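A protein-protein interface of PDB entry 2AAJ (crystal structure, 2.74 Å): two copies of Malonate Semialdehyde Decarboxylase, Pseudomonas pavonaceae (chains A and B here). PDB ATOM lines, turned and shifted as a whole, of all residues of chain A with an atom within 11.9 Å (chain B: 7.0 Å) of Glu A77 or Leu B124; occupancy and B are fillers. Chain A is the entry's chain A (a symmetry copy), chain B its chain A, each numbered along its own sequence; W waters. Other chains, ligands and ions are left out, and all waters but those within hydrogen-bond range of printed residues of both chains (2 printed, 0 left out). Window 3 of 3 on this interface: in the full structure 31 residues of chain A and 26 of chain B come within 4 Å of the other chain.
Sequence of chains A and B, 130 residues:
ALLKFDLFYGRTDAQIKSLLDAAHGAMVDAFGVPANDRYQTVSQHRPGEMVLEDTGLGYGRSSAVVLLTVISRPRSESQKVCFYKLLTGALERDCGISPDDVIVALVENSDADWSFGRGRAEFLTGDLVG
No position is printed for both chains.
Of the 13 pairs that touch across the chains among the printed residues, none has its exchanged pair printed and touching as well.
Among the printed residues, merely in contact across the chains: Leu A57 with Asp B127 (3.8 Å), Leu A57 with Leu B128 (3.7 Å), Glu A77 with Leu B124 (3.8 Å), Lys A80 with Ala B112 (3.8 Å), Val A81 with Leu B124 (3.9 Å), Tyr A84 with Asp B113 (3.4 Å), Tyr A84 with Trp B114 (3.7 Å), Val A104 with Asp B113 (3.9 Å) and Val A104 with Trp B114 (3.5 Å).
Of chain B, only Leu B124 (3.8 Å) comes within 4 Å of Glu A77.
No residue of chain A comes within 4 Å of Asp B111.
Ala B112 touches just these residues of chain A: Lys A80 and Tyr A84.
Ala B121 touches none of the printed residues of chain A.
Of the printed residues of chain A, Glu B122 touches Tyr A59.
No residue of chain A comes within 4 Å of Phe B123.
Of chain A, only Glu A77 (3.8 Å) and Val A81 (3.9 Å) come within 4 Å of Leu B124.
Thr B125 touches none of the printed residues of chain A.
No residue of chain A comes within 4 Å of Gly B126.
Of the printed residues of chain A, Leu B128 touches Leu A57.
The nearest residue of chain B that does not touch Glu A77 is Ala B112 (4.5 Å).
The nearest residue of chain A that does not touch Leu B124 is Tyr A84 (6.0 Å).
N of Leu B128 lies within hydrogen-bond range of O of Glu B122, 3.0 Å away.
The backbone NH (N) of Ser B110 lies within hydrogen-bond range of the side-chain carboxylate (OD2) of Asp B113 (2.9 Å).
The side-chain amino group (NZ) of Lys A80 is in salt-bridge range of the side-chain carboxylate (OE2) of Glu A108 (2.8 Å).
O of Glu B122 lies within hydrogen-bond range of N of Asp B127.
OG1 of Thr B125 sits at hydrogen-bond distance from N of Asp B127 (3.3 Å).
The backbone carbonyl oxygen (O) of Ala B112 sits at hydrogen-bond distance from the side-chain hydroxyl (OH) of Tyr A84 (2.8 Å).
The side-chain amino group (NZ) of Lys A80 lies within salt-bridge range of the side-chain carboxylate (OD1) of Asp B113, 2.8 Å away.
The backbone NH of Leu A106 is in hydrogen-bond range of the backbone carbonyl oxygen of Asp B113 (2.7 Å).
The side-chain hydroxyl (OH) of Tyr A59 lies within hydrogen-bond range of the side-chain carboxylate (OE2) of Glu B122 (2.6 Å).
Of the 23 printed residues of chain A, 8 touch a printed residue of chain B.
Printed residues of chain A that touch a printed residue of chain B: Leu A57, Tyr A59, Glu A77, Lys A80, Val A81, Tyr A84, Val A104 and Leu A106.
Printed residues of chain B that touch a printed residue of chain A: Ala B112, Asp B113, Trp B114, Glu B122, Leu B124, Asp B127 and Leu B128.
Hydrophobic or aromatic side chains of chain B that line the printed part of chain A: Leu B124 and Leu B128.
Among the printed residues, 13 pairs touch across the chains.
Among the printed residues, Asp or Glu carboxylates within 4 Å of a Lys or Arg side-chain nitrogen of the other chain: Lys A80 with Asp B113.
Water W2 lies within hydrogen-bond range of OH of Tyr A59 (2.7 Å) and OD2 of Asp B127 (2.8 Å).
Water W1 lies within hydrogen-bond range of the side-chain carboxylate (OD2) of Asp B113, the side-chain carboxylate (OE1) of Glu A108 and the side-chain amino group (NZ) of Lys A80.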
ATOM      1  N   ASP A  29      24.553  -8.197   9.908  1.00  0.00           N
ATOM      2  CA  ASP A  29      24.118  -8.988  11.050  1.00  0.00           C
ATOM      3  C   ASP A  29      23.275  -8.192  12.063  1.00  0.00           C
ATOM      4  O   ASP A  29      22.238  -8.691  12.527  1.00  0.00           O
ATOM      5  CB  ASP A  29      25.316  -9.665  11.750  1.00  0.00           C
ATOM      6  CG  ASP A  29      25.916 -10.796  10.924  1.00  0.00           C
ATOM      7  OD1 ASP A  29      25.212 -11.288  10.017  1.00  0.00           O
ATOM      8  OD2 ASP A  29      27.071 -11.245  11.104  1.00  0.00           O
ATOM      9  N   ALA A  30      23.687  -6.971  12.421  1.00  0.00           N
ATOM     10  CA  ALA A  30      22.926  -6.223  13.441  1.00  0.00           C
ATOM     11  C   ALA A  30      21.523  -5.807  12.945  1.00  0.00           C
ATOM     12  O   ALA A  30      20.546  -5.810  13.705  1.00  0.00           O
ATOM     13  CB  ALA A  30      23.696  -5.049  13.954  1.00  0.00           C
ATOM     14  N   PHE A  31      21.420  -5.495  11.657  1.00  0.00           N
ATOM     15  CA  PHE A  31      20.203  -4.882  11.128  1.00  0.00           C
ATOM     16  C   PHE A  31      19.382  -5.816  10.255  1.00  0.00           C
ATOM     17  O   PHE A  31      18.300  -5.437   9.826  1.00  0.00           O
ATOM     18  CB  PHE A  31      20.542  -3.612  10.340  1.00  0.00           C
ATOM     19  CG  PHE A  31      21.110  -2.483  11.177  1.00  0.00           C
ATOM     20  CD1 PHE A  31      21.048  -2.513  12.587  1.00  0.00           C
ATOM     21  CD2 PHE A  31      21.682  -1.360  10.557  1.00  0.00           C
ATOM     22  CE1 PHE A  31      21.569  -1.446  13.384  1.00  0.00           C
ATOM     23  CE2 PHE A  31      22.194  -0.287  11.329  1.00  0.00           C
ATOM     24  CZ  PHE A  31      22.142  -0.345  12.766  1.00  0.00           C
ATOM     25  N   LEU A  57      35.995   9.920  28.940  1.00  0.00           N
ATOM     26  CA  LEU A  57      35.717   8.494  29.082  1.00  0.00           C
ATOM     27  C   LEU A  57      36.995   7.596  29.157  1.00  0.00           C
ATOM     28  O   LEU A  57      36.901   6.395  29.421  1.00  0.00           O
ATOM     29  CB  LEU A  57      34.851   8.077  27.907  1.00  0.00           C
ATOM     30  CG  LEU A  57      33.323   7.978  27.917  1.00  0.00           C
ATOM     31  CD1 LEU A  57      32.600   8.341  29.202  1.00  0.00           C
ATOM     32  CD2 LEU A  57      32.664   8.669  26.735  1.00  0.00           C
ATOM     33  N   TYR A  59      39.321   6.662  26.757  1.00  0.00           N
ATOM     34  CA  TYR A  59      39.843   6.008  25.535  1.00  0.00           C
ATOM     35  C   TYR A  59      41.008   6.915  25.045  1.00  0.00           C
ATOM     36  O   TYR A  59      40.758   8.113  24.927  1.00  0.00           O
ATOM     37  CB  TYR A  59      38.736   6.033  24.480  1.00  0.00           C
ATOM     38  CG  TYR A  59      37.303   5.691  24.927  1.00  0.00           C
ATOM     39  CD1 TYR A  59      37.045   4.662  25.818  1.00  0.00           C
ATOM     40  CD2 TYR A  59      36.211   6.374  24.421  1.00  0.00           C
ATOM     41  CE1 TYR A  59      35.724   4.340  26.207  1.00  0.00           C
ATOM     42  CE2 TYR A  59      34.910   6.062  24.793  1.00  0.00           C
ATOM     43  CZ  TYR A  59      34.661   5.035  25.679  1.00  0.00           C
ATOM     44  OH  TYR A  59      33.366   4.696  26.071  1.00  0.00           O
ATOM     45  N   SER A  72      20.283   5.939   8.230  1.00  0.00           N
ATOM     46  CA  SER A  72      19.545   4.719   8.316  1.00  0.00           C
ATOM     47  C   SER A  72      18.054   4.944   8.444  1.00  0.00           C
ATOM     48  O   SER A  72      17.633   5.906   9.060  1.00  0.00           O
ATOM     49  CB  SER A  72      20.054   3.960   9.538  1.00  0.00           C
ATOM     50  OG  SER A  72      19.414   2.703   9.643  1.00  0.00           O
ATOM     51  N   ARG A  73      17.271   4.048   7.855  1.00  0.00           N
ATOM     52  CA  ARG A  73      15.861   3.902   8.142  1.00  0.00           C
ATOM     53  C   ARG A  73      15.775   3.571   9.623  1.00  0.00           C
ATOM     54  O   ARG A  73      16.812   3.211  10.169  1.00  0.00           O
ATOM     55  CB  ARG A  73      15.363   2.721   7.337  1.00  0.00           C
ATOM     56  CG  ARG A  73      14.197   3.081   6.503  1.00  0.00           C
ATOM     57  CD  ARG A  73      14.074   2.279   5.246  1.00  0.00           C
ATOM     58  NE  ARG A  73      14.138   0.820   5.466  1.00  0.00           N
ATOM     59  CZ  ARG A  73      13.078  -0.007   5.488  1.00  0.00           C
ATOM     60  NH1 ARG A  73      11.831   0.432   5.326  1.00  0.00           N
ATOM     61  NH2 ARG A  73      13.270  -1.293   5.685  1.00  0.00           N
ATOM     62  N   PRO A  74      14.607   3.682  10.301  1.00  0.00           N
ATOM     63  CA  PRO A  74      14.572   3.453  11.767  1.00  0.00           C
ATOM     64  C   PRO A  74      14.950   2.011  12.203  1.00  0.00           C
ATOM     65  O   PRO A  74      14.719   1.062  11.465  1.00  0.00           O
ATOM     66  CB  PRO A  74      13.131   3.820  12.169  1.00  0.00           C
ATOM     67  CG  PRO A  74      12.608   4.591  11.027  1.00  0.00           C
ATOM     68  CD  PRO A  74      13.263   4.033   9.786  1.00  0.00           C
ATOM     69  N   ARG A  75      15.578   1.897  13.377  1.00  0.00           N
ATOM     70  CA  ARG A  75      16.040   0.647  13.970  1.00  0.00           C
ATOM     71  C   ARG A  75      15.740   0.723  15.465  1.00  0.00           C
ATOM     72  O   ARG A  75      15.806   1.801  16.064  1.00  0.00           O
ATOM     73  CB  ARG A  75      17.551   0.487  13.805  1.00  0.00           C
ATOM     74  CG  ARG A  75      18.072   0.608  12.405  1.00  0.00           C
ATOM     75  CD  ARG A  75      17.830  -0.610  11.514  1.00  0.00           C
ATOM     76  NE  ARG A  75      18.156  -0.320  10.113  1.00  0.00           N
ATOM     77  CZ  ARG A  75      17.591  -0.956   9.074  1.00  0.00           C
ATOM     78  NH1 ARG A  75      16.680  -1.913   9.314  1.00  0.00           N
ATOM     79  NH2 ARG A  75      17.918  -0.633   7.799  1.00  0.00           N
ATOM     80  N   SER A  76      15.439  -0.433  16.067  1.00  0.00           N
ATOM     81  CA  SER A  76      15.175  -0.527  17.506  1.00  0.00           C
ATOM     82  C   SER A  76      16.434  -0.193  18.296  1.00  0.00           C
ATOM     83  O   SER A  76      17.554  -0.359  17.792  1.00  0.00           O
ATOM     84  CB  SER A  76      14.664  -1.930  17.879  1.00  0.00           C
ATOM     85  OG  SER A  76      15.691  -2.923  17.796  1.00  0.00           O
ATOM     86  N   GLU A  77      16.260   0.269  19.527  1.00  0.00           N
ATOM     87  CA  GLU A  77      17.399   0.586  20.355  1.00  0.00           C
ATOM     88  C   GLU A  77      18.285  -0.653  20.558  1.00  0.00           C
ATOM     89  O   GLU A  77      19.507  -0.545  20.662  1.00  0.00           O
ATOM     90  CB  GLU A  77      16.909   1.173  21.659  1.00  0.00           C
ATOM     91  CG  GLU A  77      17.909   1.099  22.767  1.00  0.00           C
ATOM     92  CD  GLU A  77      17.391   1.736  24.050  1.00  0.00           C
ATOM     93  OE1 GLU A  77      16.818   2.865  24.018  1.00  0.00           O
ATOM     94  OE2 GLU A  77      17.598   1.101  25.112  1.00  0.00           O
ATOM     95  N   SER A  78      17.659  -1.829  20.594  1.00  0.00           N
ATOM     96  CA  SER A  78      18.378  -3.110  20.629  1.00  0.00           C
ATOM     97  C   SER A  78      19.293  -3.386  19.450  1.00  0.00           C
ATOM     98  O   SER A  78      20.384  -3.930  19.617  1.00  0.00           O
ATOM     99  CB  SER A  78      17.383  -4.250  20.621  1.00  0.00           C
ATOM    100  OG  SER A  78      16.932  -4.402  21.939  1.00  0.00           O
ATOM    101  N   GLN A  79      18.810  -3.059  18.260  1.00  0.00           N
ATOM    102  CA  GLN A  79      19.561  -3.275  17.057  1.00  0.00           C
ATOM    103  C   GLN A  79      20.821  -2.421  17.008  1.00  0.00           C
ATOM    104  O   GLN A  79      21.892  -2.883  16.577  1.00  0.00           O
ATOM    105  CB  GLN A  79      18.675  -3.024  15.864  1.00  0.00           C
ATOM    106  CG  GLN A  79      17.688  -4.208  15.602  1.00  0.00           C
ATOM    107  CD  GLN A  79      16.822  -3.973  14.358  1.00  0.00           C
ATOM    108  OE1 GLN A  79      16.228  -2.906  14.190  1.00  0.00           O
ATOM    109  NE2 GLN A  79      16.781  -4.945  13.485  1.00  0.00           N
ATOM    110  N   LYS A  80      20.707  -1.188  17.494  1.00  0.00           N
ATOM    111  CA  LYS A  80      21.816  -0.257  17.510  1.00  0.00           C
ATOM    112  C   LYS A  80      22.893  -0.684  18.499  1.00  0.00           C
ATOM    113  O   LYS A  80      24.080  -0.801  18.123  1.00  0.00           O
ATOM    114  CB  LYS A  80      21.308   1.128  17.850  1.00  0.00           C
ATOM    115  CG  LYS A  80      20.575   1.803  16.734  1.00  0.00           C
ATOM    116  CD  LYS A  80      19.827   2.987  17.273  1.00  0.00           C
ATOM    117  CE  LYS A  80      18.722   3.356  16.303  1.00  0.00           C
ATOM    118  NZ  LYS A  80      17.986   4.563  16.770  1.00  0.00           N
ATOM    119  N   VAL A  81      22.475  -0.935  19.744  1.00  0.00           N
ATOM    120  CA  VAL A  81      23.338  -1.529  20.756  1.00  0.00           C
ATOM    121  C   VAL A  81      24.126  -2.728  20.225  1.00  0.00           C
ATOM    122  O   VAL A  81      25.347  -2.784  20.353  1.00  0.00           O
ATOM    123  CB  VAL A  81      22.524  -1.880  21.991  1.00  0.00           C
ATOM    124  CG1 VAL A  81      23.328  -2.688  22.981  1.00  0.00           C
ATOM    125  CG2 VAL A  81      22.070  -0.596  22.673  1.00  0.00           C
ATOM    126  N   CYS A  82      23.419  -3.660  19.602  1.00  0.00           N
ATOM    127  CA  CYS A  82      24.017  -4.824  18.968  1.00  0.00           C
ATOM    128  C   CYS A  82      25.039  -4.400  17.926  1.00  0.00           C
ATOM    129  O   CYS A  82      26.184  -4.868  17.942  1.00  0.00           O
ATOM    130  CB  CYS A  82      22.898  -5.641  18.347  1.00  0.00           C
ATOM    131  SG  CYS A  82      23.357  -7.213  17.650  1.00  0.00           S
ATOM    132  N   PHE A  83      24.633  -3.475  17.048  1.00  0.00           N
ATOM    133  CA  PHE A  83      25.509  -2.965  15.985  1.00  0.00           C
ATOM    134  C   PHE A  83      26.878  -2.475  16.478  1.00  0.00           C
ATOM    135  O   PHE A  83      27.906  -2.902  15.923  1.00  0.00           O
ATOM    136  CB  PHE A  83      24.836  -1.901  15.096  1.00  0.00           C
ATOM    137  CG  PHE A  83      25.773  -1.293  14.073  1.00  0.00           C
ATOM    138  CD1 PHE A  83      26.427  -2.099  13.124  1.00  0.00           C
ATOM    139  CD2 PHE A  83      26.068   0.078  14.113  1.00  0.00           C
ATOM    140  CE1 PHE A  83      27.326  -1.553  12.176  1.00  0.00           C
ATOM    141  CE2 PHE A  83      26.957   0.662  13.196  1.00  0.00           C
ATOM    142  CZ  PHE A  83      27.588  -0.164  12.198  1.00  0.00           C
ATOM    143  N   TYR A  84      26.896  -1.611  17.495  1.00  0.00           N
ATOM    144  CA  TYR A  84      28.144  -1.070  17.990  1.00  0.00           C
ATOM    145  C   TYR A  84      29.072  -2.147  18.492  1.00  0.00           C
ATOM    146  O   TYR A  84      30.273  -2.055  18.200  1.00  0.00           O
ATOM    147  CB  TYR A  84      27.937  -0.037  19.097  1.00  0.00           C
ATOM    148  CG  TYR A  84      26.942   1.039  18.778  1.00  0.00           C
ATOM    149  CD1 TYR A  84      26.936   1.656  17.524  1.00  0.00           C
ATOM    150  CD2 TYR A  84      25.973   1.431  19.714  1.00  0.00           C
ATOM    151  CE1 TYR A  84      26.020   2.638  17.204  1.00  0.00           C
ATOM    152  CE2 TYR A  84      25.003   2.435  19.388  1.00  0.00           C
ATOM    153  CZ  TYR A  84      25.046   3.034  18.129  1.00  0.00           C
ATOM    154  OH  TYR A  84      24.130   4.025  17.756  1.00  0.00           O
ATOM    155  N   LYS A  85      28.566  -3.150  19.242  1.00  0.00           N
ATOM    156  CA  LYS A  85      29.451  -4.217  19.763  1.00  0.00           C
ATOM    157  C   LYS A  85      29.920  -5.134  18.641  1.00  0.00           C
ATOM    158  O   LYS A  85      31.064  -5.621  18.642  1.00  0.00           O
ATOM    159  CB  LYS A  85      28.803  -5.094  20.841  1.00  0.00           C
ATOM    160  CG  LYS A  85      28.490  -4.368  22.109  1.00  0.00           C
ATOM    161  CD  LYS A  85      29.725  -4.129  23.063  1.00  0.00           C
ATOM    162  CE  LYS A  85      29.198  -3.519  24.465  1.00  0.00           C
ATOM    163  NZ  LYS A  85      27.643  -3.847  24.778  1.00  0.00           N
ATOM    164  N   LEU A  86      29.010  -5.413  17.717  1.00  0.00           N
ATOM    165  CA  LEU A  86      29.333  -6.226  16.572  1.00  0.00           C
ATOM    166  C   LEU A  86      30.399  -5.515  15.720  1.00  0.00           C
ATOM    167  O   LEU A  86      31.342  -6.142  15.187  1.00  0.00           O
ATOM    168  CB  LEU A  86      28.051  -6.472  15.778  1.00  0.00           C
ATOM    169  CG  LEU A  86      27.442  -7.886  15.644  1.00  0.00           C
ATOM    170  CD1 LEU A  86      27.844  -8.780  16.769  1.00  0.00           C
ATOM    171  CD2 LEU A  86      25.928  -7.864  15.496  1.00  0.00           C
ATOM    172  N   VAL A 104      31.017   6.165  16.512  1.00  0.00           N
ATOM    173  CA  VAL A 104      29.834   6.039  15.656  1.00  0.00           C
ATOM    174  C   VAL A 104      28.750   7.068  16.057  1.00  0.00           C
ATOM    175  O   VAL A 104      28.389   7.204  17.246  1.00  0.00           O
ATOM    176  CB  VAL A 104      29.153   4.640  15.776  1.00  0.00           C
ATOM    177  CG1 VAL A 104      28.114   4.450  14.693  1.00  0.00           C
ATOM    178  CG2 VAL A 104      30.129   3.528  15.815  1.00  0.00           C
ATOM    179  N   LEU A 106      24.786   8.211  14.606  1.00  0.00           N
ATOM    180  CA  LEU A 106      23.820   7.647  13.685  1.00  0.00           C
ATOM    181  C   LEU A 106      22.669   8.596  13.483  1.00  0.00           C
ATOM    182  O   LEU A 106      22.269   9.272  14.411  1.00  0.00           O
ATOM    183  CB  LEU A 106      23.417   6.261  14.184  1.00  0.00           C
ATOM    184  CG  LEU A 106      22.123   5.512  13.898  1.00  0.00           C
ATOM    185  CD1 LEU A 106      21.699   5.420  12.476  1.00  0.00           C
ATOM    186  CD2 LEU A 106      22.511   4.138  14.328  1.00  0.00           C
ATOM    187  N   GLU A 108      18.663   9.011  11.652  1.00  0.00           N
ATOM    188  CA  GLU A 108      17.527   8.265  11.088  1.00  0.00           C
ATOM    189  C   GLU A 108      16.725   9.092  10.121  1.00  0.00           C
ATOM    190  O   GLU A 108      16.549  10.316  10.302  1.00  0.00           O
ATOM    191  CB  GLU A 108      16.591   7.763  12.155  1.00  0.00           C
ATOM    192  CG  GLU A 108      17.242   6.766  13.097  1.00  0.00           C
ATOM    193  CD  GLU A 108      16.242   5.851  13.829  1.00  0.00           C
ATOM    194  OE1 GLU A 108      14.999   6.170  13.890  1.00  0.00           O
ATOM    195  OE2 GLU A 108      16.733   4.810  14.326  1.00  0.00           O
ATOM    196  N   SER B 110      19.265  10.917  18.676  1.00  0.00           N
ATOM    197  CA  SER B 110      18.846  10.607  20.030  1.00  0.00           C
ATOM    198  C   SER B 110      19.956   9.935  20.855  1.00  0.00           C
ATOM    199  O   SER B 110      21.040   9.687  20.358  1.00  0.00           O
ATOM    200  CB  SER B 110      17.605   9.731  19.966  1.00  0.00           C
ATOM    201  OG  SER B 110      17.972   8.400  19.600  1.00  0.00           O
ATOM    202  N   ASP B 111      19.700   9.657  22.119  1.00  0.00           N
ATOM    203  CA  ASP B 111      20.715   9.073  22.981  1.00  0.00           C
ATOM    204  C   ASP B 111      21.266   7.715  22.476  1.00  0.00           C
ATOM    205  O   ASP B 111      22.402   7.328  22.765  1.00  0.00           O
ATOM    206  CB  ASP B 111      20.129   8.867  24.388  1.00  0.00           C
ATOM    207  CG  ASP B 111      19.875  10.165  25.138  1.00  0.00           C
ATOM    208  OD1 ASP B 111      20.166  11.263  24.605  1.00  0.00           O
ATOM    209  OD2 ASP B 111      19.362  10.180  26.291  1.00  0.00           O
ATOM    210  N   ALA B 112      20.414   6.982  21.767  1.00  0.00           N
ATOM    211  CA  ALA B 112      20.724   5.650  21.280  1.00  0.00           C
ATOM    212  C   ALA B 112      21.666   5.716  20.082  1.00  0.00           C
ATOM    213  O   ALA B 112      22.249   4.714  19.697  1.00  0.00           O
ATOM    214  CB  ALA B 112      19.408   4.900  20.919  1.00  0.00           C
ATOM    215  N   ASP B 113      21.840   6.914  19.533  1.00  0.00           N
ATOM    216  CA  ASP B 113      22.479   7.081  18.249  1.00  0.00           C
ATOM    217  C   ASP B 113      23.958   7.421  18.320  1.00  0.00           C
ATOM    218  O   ASP B 113      24.521   7.861  17.316  1.00  0.00           O
ATOM    219  CB  ASP B 113      21.713   8.135  17.432  1.00  0.00           C
ATOM    220  CG  ASP B 113      20.256   7.738  17.146  1.00  0.00           C
ATOM    221  OD1 ASP B 113      19.968   6.522  17.033  1.00  0.00           O
ATOM    222  OD2 ASP B 113      19.327   8.577  17.015  1.00  0.00           O
ATOM    223  N   TRP B 114      24.570   7.223  19.486  1.00  0.00           N
ATOM    224  CA  TRP B 114      25.974   7.566  19.721  1.00  0.00           C
ATOM    225  C   TRP B 114      26.714   6.435  20.420  1.00  0.00           C
ATOM    226  O   TRP B 114      26.183   5.786  21.350  1.00  0.00           O
ATOM    227  CB  TRP B 114      26.101   8.801  20.580  1.00  0.00           C
ATOM    228  CG  TRP B 114      25.544  10.023  19.932  1.00  0.00           C
ATOM    229  CD1 TRP B 114      24.252  10.497  20.020  1.00  0.00           C
ATOM    230  CD2 TRP B 114      26.248  10.956  19.093  1.00  0.00           C
ATOM    231  NE1 TRP B 114      24.121  11.657  19.291  1.00  0.00           N
ATOM    232  CE2 TRP B 114      25.332  11.969  18.722  1.00  0.00           C
ATOM    233  CE3 TRP B 114      27.573  11.047  18.626  1.00  0.00           C
ATOM    234  CZ2 TRP B 114      25.693  13.041  17.886  1.00  0.00           C
ATOM    235  CZ3 TRP B 114      27.934  12.122  17.832  1.00  0.00           C
ATOM    236  CH2 TRP B 114      26.996  13.093  17.450  1.00  0.00           C
ATOM    237  N   ALA B 121      27.142   2.144  24.030  1.00  0.00           N
ATOM    238  CA  ALA B 121      26.194   3.266  23.873  1.00  0.00           C
ATOM    239  C   ALA B 121      26.122   4.106  25.174  1.00  0.00           C
ATOM    240  O   ALA B 121      25.237   3.887  26.011  1.00  0.00           O
ATOM    241  CB  ALA B 121      24.822   2.733  23.498  1.00  0.00           C
ATOM    242  N   GLU B 122      27.043   5.052  25.357  1.00  0.00           N
ATOM    243  CA  GLU B 122      27.244   5.689  26.672  1.00  0.00           C
ATOM    244  C   GLU B 122      26.077   6.492  27.231  1.00  0.00           C
ATOM    245  O   GLU B 122      25.985   6.688  28.451  1.00  0.00           O
ATOM    246  CB  GLU B 122      28.507   6.544  26.700  1.00  0.00           C
ATOM    247  CG  GLU B 122      29.743   5.732  26.385  1.00  0.00           C
ATOM    248  CD  GLU B 122      30.149   5.765  24.925  1.00  0.00           C
ATOM    249  OE1 GLU B 122      29.307   6.107  24.065  1.00  0.00           O
ATOM    250  OE2 GLU B 122      31.321   5.458  24.652  1.00  0.00           O
ATOM    251  N   PHE B 123      25.197   6.970  26.365  1.00  0.00           N
ATOM    252  CA  PHE B 123      24.054   7.698  26.850  1.00  0.00           C
ATOM    253  C   PHE B 123      23.033   6.738  27.434  1.00  0.00           C
ATOM    254  O   PHE B 123      22.351   7.077  28.384  1.00  0.00           O
ATOM    255  CB  PHE B 123      23.443   8.555  25.747  1.00  0.00           C
ATOM    256  CG  PHE B 123      24.288   9.749  25.362  1.00  0.00           C
ATOM    257  CD1 PHE B 123      24.688  10.685  26.330  1.00  0.00           C
ATOM    258  CD2 PHE B 123      24.693   9.939  24.035  1.00  0.00           C
ATOM    259  CE1 PHE B 123      25.471  11.801  25.964  1.00  0.00           C
ATOM    260  CE2 PHE B 123      25.479  11.037  23.666  1.00  0.00           C
ATOM    261  CZ  PHE B 123      25.867  11.965  24.626  1.00  0.00           C
ATOM    262  N   LEU B 124      22.946   5.543  26.856  1.00  0.00           N
ATOM    263  CA  LEU B 124      22.054   4.461  27.269  1.00  0.00           C
ATOM    264  C   LEU B 124      22.562   3.731  28.548  1.00  0.00           C
ATOM    265  O   LEU B 124      21.764   3.492  29.492  1.00  0.00           O
ATOM    266  CB  LEU B 124      21.921   3.469  26.119  1.00  0.00           C
ATOM    267  CG  LEU B 124      20.720   3.518  25.189  1.00  0.00           C
ATOM    268  CD1 LEU B 124      20.169   4.889  25.068  1.00  0.00           C
ATOM    269  CD2 LEU B 124      21.090   2.962  23.843  1.00  0.00           C
ATOM    270  N   THR B 125      23.863   3.374  28.587  1.00  0.00           N
ATOM    271  CA  THR B 125      24.431   2.732  29.774  1.00  0.00           C
ATOM    272  C   THR B 125      24.535   3.698  30.916  1.00  0.00           C
ATOM    273  O   THR B 125      24.582   3.262  32.039  1.00  0.00           O
ATOM    274  CB  THR B 125      25.823   2.156  29.560  1.00  0.00           C
ATOM    275  OG1 THR B 125      26.761   3.232  29.414  1.00  0.00           O
ATOM    276  CG2 THR B 125      25.902   1.290  28.289  1.00  0.00           C
ATOM    277  N   GLY B 126      24.603   4.998  30.635  1.00  0.00           N
ATOM    278  CA  GLY B 126      24.644   6.021  31.667  1.00  0.00           C
ATOM    279  C   GLY B 126      26.051   6.449  32.039  1.00  0.00           C
ATOM    280  O   GLY B 126      26.207   7.230  32.964  1.00  0.00           O
ATOM    281  N   ASP B 127      27.075   5.942  31.340  1.00  0.00           N
ATOM    282  CA  ASP B 127      28.430   6.508  31.378  1.00  0.00           C
ATOM    283  C   ASP B 127      28.505   8.000  31.037  1.00  0.00           C
ATOM    284  O   ASP B 127      29.489   8.634  31.409  1.00  0.00           O
ATOM    285  CB  ASP B 127      29.322   5.790  30.389  1.00  0.00           C
ATOM    286  CG  ASP B 127      29.812   4.501  30.904  1.00  0.00           C
ATOM    287  OD1 ASP B 127      29.566   4.222  32.075  1.00  0.00           O
ATOM    288  OD2 ASP B 127      30.456   3.696  30.214  1.00  0.00           O
ATOM    289  N   LEU B 128      27.527   8.516  30.267  1.00  0.00           N
ATOM    290  CA  LEU B 128      27.295   9.959  30.048  1.00  0.00           C
ATOM    291  C   LEU B 128      25.819  10.296  30.242  1.00  0.00           C
ATOM    292  O   LEU B 128      24.930   9.435  30.026  1.00  0.00           O
ATOM    293  CB  LEU B 128      27.705  10.416  28.650  1.00  0.00           C
ATOM    294  CG  LEU B 128      29.127  10.281  28.124  1.00  0.00           C
ATOM    295  CD1 LEU B 128      29.120  10.695  26.672  1.00  0.00           C
ATOM    296  CD2 LEU B 128      30.146  11.065  28.929  1.00  0.00           C
HETATM  297  O   HOH W   1      16.716   7.648  16.054  1.00  0.00           O
HETATM  298  O   HOH W   2      32.706   3.911  28.525  1.00  0.00           O
